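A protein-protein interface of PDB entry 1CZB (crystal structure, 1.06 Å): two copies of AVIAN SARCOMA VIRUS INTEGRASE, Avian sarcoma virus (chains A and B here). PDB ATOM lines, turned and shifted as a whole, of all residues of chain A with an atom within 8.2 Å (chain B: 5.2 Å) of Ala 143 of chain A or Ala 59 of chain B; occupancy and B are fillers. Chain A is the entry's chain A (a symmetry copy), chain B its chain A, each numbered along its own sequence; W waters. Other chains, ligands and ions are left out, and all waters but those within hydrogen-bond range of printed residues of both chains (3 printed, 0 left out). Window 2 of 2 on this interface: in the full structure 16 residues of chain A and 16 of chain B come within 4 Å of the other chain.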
ATOM      1  N   MET A  24      25.952 -24.854  33.838  1.00  0.00           N
ATOM      2  CA  MET A  24      27.207 -24.167  34.011  1.00  0.00           C
ATOM      3  C   MET A  24      28.247 -24.953  34.840  1.00  0.00           C
ATOM      4  O   MET A  24      29.281 -24.413  35.216  1.00  0.00           O
ATOM      5  CB  MET A  24      26.941 -22.811  34.668  1.00  0.00           C
ATOM      6  CG  MET A  24      26.257 -21.825  33.702  1.00  0.00           C
ATOM      7  SD  MET A  24      27.441 -21.094  32.571  1.00  0.00           S
ATOM      8  CE  MET A  24      26.345 -20.193  31.477  1.00  0.00           C
ATOM      9  N   VAL A  43      26.039 -11.151  37.249  1.00  0.00           N
ATOM     10  CA  VAL A  43      26.162 -12.574  37.572  1.00  0.00           C
ATOM     11  C   VAL A  43      27.570 -13.017  37.359  1.00  0.00           C
ATOM     12  O   VAL A  43      28.207 -12.641  36.388  1.00  0.00           O
ATOM     13  CB  VAL A  43      25.174 -13.439  36.736  1.00  0.00           C
ATOM     14  CG1 VAL A  43      25.363 -13.236  35.245  1.00  0.00           C
ATOM     15  CG2 VAL A  43      25.252 -14.884  37.140  1.00  0.00           C
ATOM     16  N   GLN A  45      30.054 -16.863  38.041  1.00  0.00           N
ATOM     17  CA  GLN A  45      29.906 -18.293  38.342  1.00  0.00           C
ATOM     18  C   GLN A  45      31.084 -18.713  39.236  1.00  0.00           C
ATOM     19  O   GLN A  45      32.189 -18.167  39.261  1.00  0.00           O
ATOM     20  CB  GLN A  45      29.747 -19.158  37.049  1.00  0.00           C
ATOM     21  CG  GLN A  45      30.955 -19.129  36.173  1.00  0.00           C
ATOM     22  CD  GLN A  45      30.778 -19.931  34.902  1.00  0.00           C
ATOM     23  OE1 GLN A  45      31.110 -19.431  33.789  1.00  0.00           O
ATOM     24  NE2 GLN A  45      30.326 -21.173  34.933  1.00  0.00           N
ATOM     25  N   LEU A 116      17.513 -15.260  34.522  1.00  0.00           N
ATOM     26  CA  LEU A 116      18.820 -15.688  34.101  1.00  0.00           C
ATOM     27  C   LEU A 116      18.838 -17.137  33.691  1.00  0.00           C
ATOM     28  O   LEU A 116      19.394 -17.487  32.663  1.00  0.00           O
ATOM     29  CB  LEU A 116      19.674 -15.398  35.407  1.00  0.00           C
ATOM     30  CG  LEU A 116      21.065 -15.800  35.032  1.00  0.00           C
ATOM     31  CD1 LEU A 116      21.791 -15.001  33.962  1.00  0.00           C
ATOM     32  CD2 LEU A 116      21.876 -15.716  36.346  1.00  0.00           C
ATOM     33  N   ILE A 120      19.789 -18.413  30.000  1.00  0.00           N
ATOM     34  CA  ILE A 120      20.879 -19.349  29.807  1.00  0.00           C
ATOM     35  C   ILE A 120      20.415 -20.561  29.013  1.00  0.00           C
ATOM     36  O   ILE A 120      21.090 -20.987  28.068  1.00  0.00           O
ATOM     37  CB  ILE A 120      21.512 -19.726  31.148  1.00  0.00           C
ATOM     38  CG1 ILE A 120      22.279 -18.542  31.757  1.00  0.00           C
ATOM     39  CG2 ILE A 120      22.396 -20.954  31.010  1.00  0.00           C
ATOM     40  CD1 ILE A 120      22.672 -18.733  33.197  1.00  0.00           C
ATOM     41  N   LEU A 123      19.759 -19.520  25.294  1.00  0.00           N
ATOM     42  CA  LEU A 123      20.984 -19.280  24.559  1.00  0.00           C
ATOM     43  C   LEU A 123      21.735 -20.600  24.315  1.00  0.00           C
ATOM     44  O   LEU A 123      22.241 -20.832  23.218  1.00  0.00           O
ATOM     45  CB  LEU A 123      21.860 -18.281  25.288  1.00  0.00           C
ATOM     46  CG  LEU A 123      21.293 -16.884  25.448  1.00  0.00           C
ATOM     47  CD1 LEU A 123      22.223 -16.060  26.342  1.00  0.00           C
ATOM     48  CD2 LEU A 123      21.102 -16.213  24.093  1.00  0.00           C
ATOM     49  N   LYS A 137      32.818 -22.790  26.540  1.00  0.00           N
ATOM     50  CA  LYS A 137      31.807 -21.908  25.973  1.00  0.00           C
ATOM     51  C   LYS A 137      31.033 -21.131  27.040  1.00  0.00           C
ATOM     52  O   LYS A 137      30.241 -20.231  26.706  1.00  0.00           O
ATOM     53  CB  LYS A 137      30.851 -22.705  25.101  1.00  0.00           C
ATOM     54  CG  LYS A 137      31.569 -23.443  23.949  1.00  0.00           C
ATOM     55  CD  LYS A 137      32.164 -22.562  22.929  1.00  0.00           C
ATOM     56  CE  LYS A 137      32.601 -23.372  21.667  1.00  0.00           C
ATOM     57  NZ  LYS A 137      33.348 -24.574  22.100  1.00  0.00           N
ATOM     58  N   GLN A 138      31.182 -21.491  28.301  1.00  0.00           N
ATOM     59  CA  GLN A 138      30.346 -20.974  29.389  1.00  0.00           C
ATOM     60  C   GLN A 138      30.543 -19.495  29.651  1.00  0.00           C
ATOM     61  O   GLN A 138      29.559 -18.801  29.877  1.00  0.00           O
ATOM     62  CB  GLN A 138      30.620 -21.728  30.683  1.00  0.00           C
ATOM     63  CG  GLN A 138      30.028 -23.167  30.629  1.00  0.00           C
ATOM     64  CD  GLN A 138      30.425 -23.948  31.860  1.00  0.00           C
ATOM     65  OE1 GLN A 138      31.024 -23.409  32.812  1.00  0.00           O
ATOM     66  NE2 GLN A 138      30.027 -25.239  31.884  1.00  0.00           N
ATOM     67  N   GLY A 139      31.780 -19.033  29.686  1.00  0.00           N
ATOM     68  CA  GLY A 139      32.023 -17.650  30.072  1.00  0.00           C
ATOM     69  C   GLY A 139      31.321 -16.696  29.143  1.00  0.00           C
ATOM     70  O   GLY A 139      30.647 -15.727  29.587  1.00  0.00           O
ATOM     71  N   GLU A 140      31.482 -16.902  27.840  1.00  0.00           N
ATOM     72  CA  GLU A 140      30.854 -16.007  26.890  1.00  0.00           C
ATOM     73  C   GLU A 140      29.326 -16.156  26.949  1.00  0.00           C
ATOM     74  O   GLU A 140      28.601 -15.177  26.754  1.00  0.00           O
ATOM     75  CB  GLU A 140      31.344 -16.193  25.452  1.00  0.00           C
ATOM     76  CG  GLU A 140      32.812 -15.775  25.311  1.00  0.00           C
ATOM     77  CD  GLU A 140      33.192 -15.477  23.857  1.00  0.00           C
ATOM     78  OE1 GLU A 140      32.279 -15.253  23.012  1.00  0.00           O
ATOM     79  OE2 GLU A 140      34.385 -15.403  23.584  1.00  0.00           O
ATOM     80  N   LEU A 141      28.818 -17.382  27.152  1.00  0.00           N
ATOM     81  CA  LEU A 141      27.354 -17.545  27.187  1.00  0.00           C
ATOM     82  C   LEU A 141      26.779 -16.832  28.414  1.00  0.00           C
ATOM     83  O   LEU A 141      25.733 -16.189  28.331  1.00  0.00           O
ATOM     84  CB  LEU A 141      27.002 -19.018  27.114  1.00  0.00           C
ATOM     85  CG  LEU A 141      25.520 -19.318  26.849  1.00  0.00           C
ATOM     86  CD1 LEU A 141      25.392 -20.627  26.140  1.00  0.00           C
ATOM     87  CD2 LEU A 141      24.680 -19.277  28.108  1.00  0.00           C
ATOM     88  N   LEU A 142      27.445 -16.962  29.568  1.00  0.00           N
ATOM     89  CA  LEU A 142      26.970 -16.271  30.768  1.00  0.00           C
ATOM     90  C   LEU A 142      26.965 -14.759  30.570  1.00  0.00           C
ATOM     91  O   LEU A 142      26.021 -14.059  30.928  1.00  0.00           O
ATOM     92  CB  LEU A 142      27.821 -16.670  31.980  1.00  0.00           C
ATOM     93  CG  LEU A 142      27.323 -16.113  33.302  1.00  0.00           C
ATOM     94  CD1 LEU A 142      25.956 -16.696  33.670  1.00  0.00           C
ATOM     95  CD2 LEU A 142      28.375 -16.390  34.370  1.00  0.00           C
ATOM     96  N   ALA A 143      28.048 -14.233  29.978  1.00  0.00           N
ATOM     97  CA  ALA A 143      28.136 -12.813  29.677  1.00  0.00           C
ATOM     98  C   ALA A 143      27.029 -12.388  28.700  1.00  0.00           C
ATOM     99  O   ALA A 143      26.490 -11.275  28.825  1.00  0.00           O
ATOM    100  CB  ALA A 143      29.497 -12.454  29.124  1.00  0.00           C
ATOM    101  N   LYS A 144      26.720 -13.227  27.749  1.00  0.00           N
ATOM    102  CA  LYS A 144      25.651 -12.954  26.779  1.00  0.00           C
ATOM    103  C   LYS A 144      24.297 -12.891  27.496  1.00  0.00           C
ATOM    104  O   LYS A 144      23.480 -12.021  27.173  1.00  0.00           O
ATOM    105  CB  LYS A 144      25.683 -13.995  25.673  1.00  0.00           C
ATOM    106  CG  LYS A 144      24.675 -13.707  24.554  1.00  0.00           C
ATOM    107  CD  LYS A 144      24.701 -14.797  23.492  1.00  0.00           C
ATOM    108  CE  LYS A 144      25.922 -14.925  22.720  1.00  0.00           C
ATOM    109  NZ  LYS A 144      25.838 -16.142  21.833  1.00  0.00           N
ATOM    110  N   ALA A 145      24.067 -13.792  28.440  1.00  0.00           N
ATOM    111  CA  ALA A 145      22.815 -13.761  29.212  1.00  0.00           C
ATOM    112  C   ALA A 145      22.706 -12.480  30.023  1.00  0.00           C
ATOM    113  O   ALA A 145      21.633 -11.875  30.092  1.00  0.00           O
ATOM    114  CB  ALA A 145      22.716 -14.994  30.088  1.00  0.00           C
ATOM    115  N   MET A 146      23.794 -12.060  30.670  1.00  0.00           N
ATOM    116  CA  MET A 146      23.798 -10.839  31.416  1.00  0.00           C
ATOM    117  C   MET A 146      23.523  -9.637  30.515  1.00  0.00           C
ATOM    118  O   MET A 146      22.690  -8.777  30.842  1.00  0.00           O
ATOM    119  CB  MET A 146      25.144 -10.672  32.134  1.00  0.00           C
ATOM    120  CG  MET A 146      25.254  -9.414  32.962  1.00  0.00           C
ATOM    121  SD  MET A 146      26.770  -9.424  33.935  1.00  0.00           S
ATOM    122  CE  MET A 146      26.958  -7.651  34.208  1.00  0.00           C
ATOM    123  N   TYR A 147      24.193  -9.569  29.361  1.00  0.00           N
ATOM    124  CA  TYR A 147      23.918  -8.540  28.371  1.00  0.00           C
ATOM    125  C   TYR A 147      22.454  -8.524  28.025  1.00  0.00           C
ATOM    126  O   TYR A 147      21.812  -7.475  27.949  1.00  0.00           O
ATOM    127  CB  TYR A 147      24.774  -8.771  27.144  1.00  0.00           C
ATOM    128  CG  TYR A 147      24.190  -8.238  25.848  1.00  0.00           C
ATOM    129  CD1 TYR A 147      24.230  -6.897  25.522  1.00  0.00           C
ATOM    130  CD2 TYR A 147      23.605  -9.099  24.924  1.00  0.00           C
ATOM    131  CE1 TYR A 147      23.688  -6.433  24.328  1.00  0.00           C
ATOM    132  CE2 TYR A 147      23.071  -8.663  23.754  1.00  0.00           C
ATOM    133  CZ  TYR A 147      23.129  -7.337  23.451  1.00  0.00           C
ATOM    134  OH  TYR A 147      22.597  -6.850  22.262  1.00  0.00           O
ATOM    135  N   ALA A 148      21.894  -9.697  27.737  1.00  0.00           N
ATOM    136  CA  ALA A 148      20.549  -9.823  27.215  1.00  0.00           C
ATOM    137  C   ALA A 148      19.533  -9.258  28.203  1.00  0.00           C
ATOM    138  O   ALA A 148      18.512  -8.684  27.804  1.00  0.00           O
ATOM    139  CB  ALA A 148      20.219 -11.275  26.925  1.00  0.00           C
ATOM    140  N   LEU A 149      19.786  -9.417  29.489  1.00  0.00           N
ATOM    141  CA  LEU A 149      18.860  -8.991  30.535  1.00  0.00           C
ATOM    142  C   LEU A 149      19.091  -7.538  30.875  1.00  0.00           C
ATOM    143  O   LEU A 149      18.120  -6.921  31.328  1.00  0.00           O
ATOM    144  CB  LEU A 149      18.974  -9.923  31.723  1.00  0.00           C
ATOM    145  CG  LEU A 149      18.555 -11.350  31.438  1.00  0.00           C
ATOM    146  CD1 LEU A 149      18.720 -12.175  32.706  1.00  0.00           C
ATOM    147  CD2 LEU A 149      17.081 -11.503  30.935  1.00  0.00           C
ATOM    148  N   ASN A 150      20.226  -6.918  30.637  1.00  0.00           N
ATOM    149  CA  ASN A 150      20.524  -5.557  31.074  1.00  0.00           C
ATOM    150  C   ASN A 150      20.415  -4.471  30.029  1.00  0.00           C
ATOM    151  O   ASN A 150      20.119  -3.334  30.373  1.00  0.00           O
ATOM    152  CB  ASN A 150      21.943  -5.455  31.636  1.00  0.00           C
ATOM    153  CG  ASN A 150      22.057  -6.150  32.990  1.00  0.00           C
ATOM    154  OD1 ASN A 150      21.086  -6.536  33.646  1.00  0.00           O
ATOM    155  ND2 ASN A 150      23.320  -6.295  33.374  1.00  0.00           N
ATOM    156  N   HIS A 151      20.711  -4.703  28.794  1.00  0.00           N
ATOM    157  CA  HIS A 151      20.998  -3.685  27.786  1.00  0.00           C
ATOM    158  C   HIS A 151      19.903  -3.766  26.764  1.00  0.00           C
ATOM    159  O   HIS A 151      19.819  -4.771  26.068  1.00  0.00           O
ATOM    160  CB  HIS A 151      22.416  -3.882  27.183  1.00  0.00           C
ATOM    161  CG  HIS A 151      23.461  -3.682  28.246  1.00  0.00           C
ATOM    162  ND1 HIS A 151      23.661  -2.442  28.860  1.00  0.00           N
ATOM    163  CD2 HIS A 151      24.382  -4.569  28.824  1.00  0.00           C
ATOM    164  CE1 HIS A 151      24.628  -2.552  29.753  1.00  0.00           C
ATOM    165  NE2 HIS A 151      25.044  -3.811  29.734  1.00  0.00           N
ATOM    166  N   ALA B  54      40.809 -11.867  23.272  1.00  0.00           N
ATOM    167  CA  ALA B  54      40.146 -10.624  22.915  1.00  0.00           C
ATOM    168  C   ALA B  54      38.632 -10.811  22.904  1.00  0.00           C
ATOM    169  O   ALA B  54      37.888  -9.948  23.367  1.00  0.00           O
ATOM    170  CB  ALA B  54      40.637 -10.132  21.568  1.00  0.00           C
ATOM    171  N   GLN B  55      38.174 -11.933  22.368  1.00  0.00           N
ATOM    172  CA  GLN B  55      36.751 -12.239  22.299  1.00  0.00           C
ATOM    173  C   GLN B  55      36.154 -12.433  23.657  1.00  0.00           C
ATOM    174  O   GLN B  55      35.067 -11.909  23.989  1.00  0.00           O
ATOM    175  CB  GLN B  55      36.563 -13.450  21.380  1.00  0.00           C
ATOM    176  CG  GLN B  55      37.006 -13.157  19.950  1.00  0.00           C
ATOM    177  CD  GLN B  55      37.261 -14.439  19.138  1.00  0.00           C
ATOM    178  OE1 GLN B  55      36.644 -15.495  19.379  1.00  0.00           O
ATOM    179  NE2 GLN B  55      38.125 -14.328  18.153  1.00  0.00           N
ATOM    180  N   HIS B  56      36.830 -13.150  24.537  1.00  0.00           N
ATOM    181  CA  HIS B  56      36.373 -13.315  25.898  1.00  0.00           C
ATOM    182  C   HIS B  56      36.270 -11.980  26.611  1.00  0.00           C
ATOM    183  O   HIS B  56      35.315 -11.701  27.351  1.00  0.00           O
ATOM    184  CB  HIS B  56      37.343 -14.218  26.638  1.00  0.00           C
ATOM    185  CG  HIS B  56      37.290 -15.646  26.312  1.00  0.00           C
ATOM    186  ND1 HIS B  56      36.453 -16.247  25.383  1.00  0.00           N
ATOM    187  CD2 HIS B  56      38.030 -16.635  26.861  1.00  0.00           C
ATOM    188  CE1 HIS B  56      36.671 -17.539  25.413  1.00  0.00           C
ATOM    189  NE2 HIS B  56      37.618 -17.814  26.273  1.00  0.00           N
ATOM    190  N   HIS B  57      37.267 -11.105  26.393  1.00  0.00           N
ATOM    191  CA  HIS B  57      37.259  -9.773  26.971  1.00  0.00           C
ATOM    192  C   HIS B  57      36.057  -8.994  26.484  1.00  0.00           C
ATOM    193  O   HIS B  57      35.336  -8.384  27.290  1.00  0.00           O
ATOM    194  CB  HIS B  57      38.558  -9.041  26.566  1.00  0.00           C
ATOM    195  CG  HIS B  57      38.475  -7.586  26.864  1.00  0.00           C
ATOM    196  ND1 HIS B  57      38.589  -7.047  28.086  1.00  0.00           N
ATOM    197  CD2 HIS B  57      38.245  -6.534  26.030  1.00  0.00           C
ATOM    198  CE1 HIS B  57      38.446  -5.726  27.987  1.00  0.00           C
ATOM    199  NE2 HIS B  57      38.235  -5.369  26.762  1.00  0.00           N
ATOM    200  N   TRP B  58      35.838  -8.938  25.165  1.00  0.00           N
ATOM    201  CA  TRP B  58      34.717  -8.159  24.657  1.00  0.00           C
ATOM    202  C   TRP B  58      33.393  -8.745  25.133  1.00  0.00           C
ATOM    203  O   TRP B  58      32.447  -7.961  25.344  1.00  0.00           O
ATOM    204  CB  TRP B  58      34.758  -8.069  23.135  1.00  0.00           C
ATOM    205  CG  TRP B  58      35.762  -7.069  22.619  1.00  0.00           C
ATOM    206  CD1 TRP B  58      36.107  -5.864  23.128  1.00  0.00           C
ATOM    207  CD2 TRP B  58      36.533  -7.223  21.435  1.00  0.00           C
ATOM    208  NE1 TRP B  58      37.048  -5.251  22.336  1.00  0.00           N
ATOM    209  CE2 TRP B  58      37.337  -6.053  21.291  1.00  0.00           C
ATOM    210  CE3 TRP B  58      36.620  -8.239  20.468  1.00  0.00           C
ATOM    211  CZ2 TRP B  58      38.207  -5.911  20.212  1.00  0.00           C
ATOM    212  CZ3 TRP B  58      37.493  -8.068  19.411  1.00  0.00           C
ATOM    213  CH2 TRP B  58      38.275  -6.919  19.297  1.00  0.00           C
ATOM    214  N   ALA B  59      33.277 -10.043  25.261  1.00  0.00           N
ATOM    215  CA  ALA B  59      32.025 -10.615  25.792  1.00  0.00           C
ATOM    216  C   ALA B  59      31.731  -9.990  27.150  1.00  0.00           C
ATOM    217  O   ALA B  59      30.601  -9.614  27.476  1.00  0.00           O
ATOM    218  CB  ALA B  59      32.104 -12.120  25.828  1.00  0.00           C
ATOM    219  N   THR B  60      32.749  -9.926  28.022  1.00  0.00           N
ATOM    220  CA  THR B  60      32.610  -9.291  29.324  1.00  0.00           C
ATOM    221  C   THR B  60      32.266  -7.806  29.185  1.00  0.00           C
ATOM    222  O   THR B  60      31.373  -7.305  29.879  1.00  0.00           O
ATOM    223  CB  THR B  60      33.884  -9.490  30.146  1.00  0.00           C
ATOM    224  OG1 THR B  60      34.106 -10.875  30.289  1.00  0.00           O
ATOM    225  CG2 THR B  60      33.797  -8.774  31.484  1.00  0.00           C
ATOM    226  N   ALA B  61      32.981  -7.092  28.325  1.00  0.00           N
ATOM    227  CA  ALA B  61      32.741  -5.679  28.166  1.00  0.00           C
ATOM    228  C   ALA B  61      31.322  -5.393  27.697  1.00  0.00           C
ATOM    229  O   ALA B  61      30.718  -4.420  28.142  1.00  0.00           O
ATOM    230  CB  ALA B  61      33.779  -5.036  27.252  1.00  0.00           C
ATOM    231  N   ILE B  62      30.777  -6.211  26.804  1.00  0.00           N
ATOM    232  CA  ILE B  62      29.391  -6.054  26.339  1.00  0.00           C
ATOM    233  C   ILE B  62      28.444  -6.272  27.478  1.00  0.00           C
ATOM    234  O   ILE B  62      27.456  -5.528  27.619  1.00  0.00           O
ATOM    235  CB  ILE B  62      29.109  -6.996  25.168  1.00  0.00           C
ATOM    236  CG1 ILE B  62      29.934  -6.594  23.927  1.00  0.00           C
ATOM    237  CG2 ILE B  62      27.648  -7.098  24.831  1.00  0.00           C
ATOM    238  CD1 ILE B  62      29.953  -7.699  22.845  1.00  0.00           C
ATOM    239  N   ALA B  63      28.670  -7.251  28.331  1.00  0.00           N
ATOM    240  CA  ALA B  63      27.846  -7.470  29.537  1.00  0.00           C
ATOM    241  C   ALA B  63      27.838  -6.240  30.419  1.00  0.00           C
ATOM    242  O   ALA B  63      26.820  -5.907  31.027  1.00  0.00           O
ATOM    243  CB  ALA B  63      28.284  -8.686  30.290  1.00  0.00           C
ATOM    244  N   TRP B  87      33.925 -12.899  14.765  1.00  0.00           N
ATOM    245  CA  TRP B  87      33.252 -12.726  16.043  1.00  0.00           C
ATOM    246  C   TRP B  87      32.583 -11.359  16.096  1.00  0.00           C
ATOM    247  O   TRP B  87      31.455 -11.189  16.554  1.00  0.00           O
ATOM    248  CB  TRP B  87      34.277 -12.926  17.173  1.00  0.00           C
ATOM    249  CG  TRP B  87      33.737 -12.964  18.546  1.00  0.00           C
ATOM    250  CD1 TRP B  87      33.472 -14.109  19.297  1.00  0.00           C
ATOM    251  CD2 TRP B  87      33.401 -11.872  19.395  1.00  0.00           C
ATOM    252  NE1 TRP B  87      32.996 -13.792  20.518  1.00  0.00           N
ATOM    253  CE2 TRP B  87      32.944 -12.423  20.632  1.00  0.00           C
ATOM    254  CE3 TRP B  87      33.452 -10.505  19.297  1.00  0.00           C
ATOM    255  CZ2 TRP B  87      32.533 -11.615  21.703  1.00  0.00           C
ATOM    256  CZ3 TRP B  87      33.041  -9.702  20.351  1.00  0.00           C
ATOM    257  CH2 TRP B  87      32.589 -10.263  21.547  1.00  0.00           C
HETATM  258  O   HOH W   1      35.166 -16.759  21.248  1.00  0.00           O
HETATM  259  O   HOH W   2      28.320 -10.562  26.181  1.00  0.00           O
HETATM  260  O   HOH W   3      34.853 -16.557  28.434  1.00  0.00           O
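ND1 of His 56 of chain B is in hydrogen-bond range of OE2 of Glu 140 of chain A (2.9 Å).
A ring nitrogen (NE2) of His 151 of chain A sits at hydrogen-bond distance from the backbone carbonyl oxygen (O) of Ala 63 of chain B, 3.0 Å away.
OE1 of Glu 140 of chain A sits at hydrogen-bond distance from NE1 of Trp 87 of chain B, at 3.0 Å.
The backbone carbonyl oxygen of His 56 of chain B sits at hydrogen-bond distance from the side-chain hydroxyl of Thr 60 of chain B, 3.3 Å away.
Among the printed residues, merely in contact across the chains: His 151 of chain A with Ile 62 of chain B (3.4 Å), Glu 140 of chain A with Gln 55 of chain B (3.5 Å), Ala 143 of chain A with Ala 59 of chain B (3.5 Å), Ala 143 of chain A with Ala 63 of chain B (3.5 Å), Tyr 147 of chain A with Ile 62 of chain B (3.5 Å), Met 146 of chain A with Ala 63 of chain B (3.6 Å) and Glu 140 of chain A with Ala 59 of chain B (3.8 Å).
Of chain B, only Ala 59 and Ala 63 come within 4 Å of Ala 143 of chain A.
Of the printed residues of chain B, Tyr 147 of chain A touches Ile 62.
Of the printed residues of chain A, Ile 62 of chain B touches Tyr 147 and His 151.
Along chain B the printed residues that touch a printed residue of chain A span positions 55 to 87.
Of the 21 printed residues of chain A, 5 touch a printed residue of chain B.
Among the printed residues, 10 pairs touch across the chains.
Among the printed residues, no Asp or Glu carboxylate lies within 4 Å of a Lys or Arg side-chain nitrogen of the other chain.
No position is printed for both chains.
Water W1 lies within hydrogen-bond range of OE1 of Gln 55 of chain B (2.7 Å) and OE2 of Glu 140 of chain A (2.8 Å).
Water W2 lies within hydrogen-bond range of O of Ala 59 of chain B, O of Ala 143 of chain A and N of Lys 144 of chain A.
Water W3 bridges the backbone NH (N) of Glu 140 of chain A and a ring nitrogen (ND1) of His 56 of chain B.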
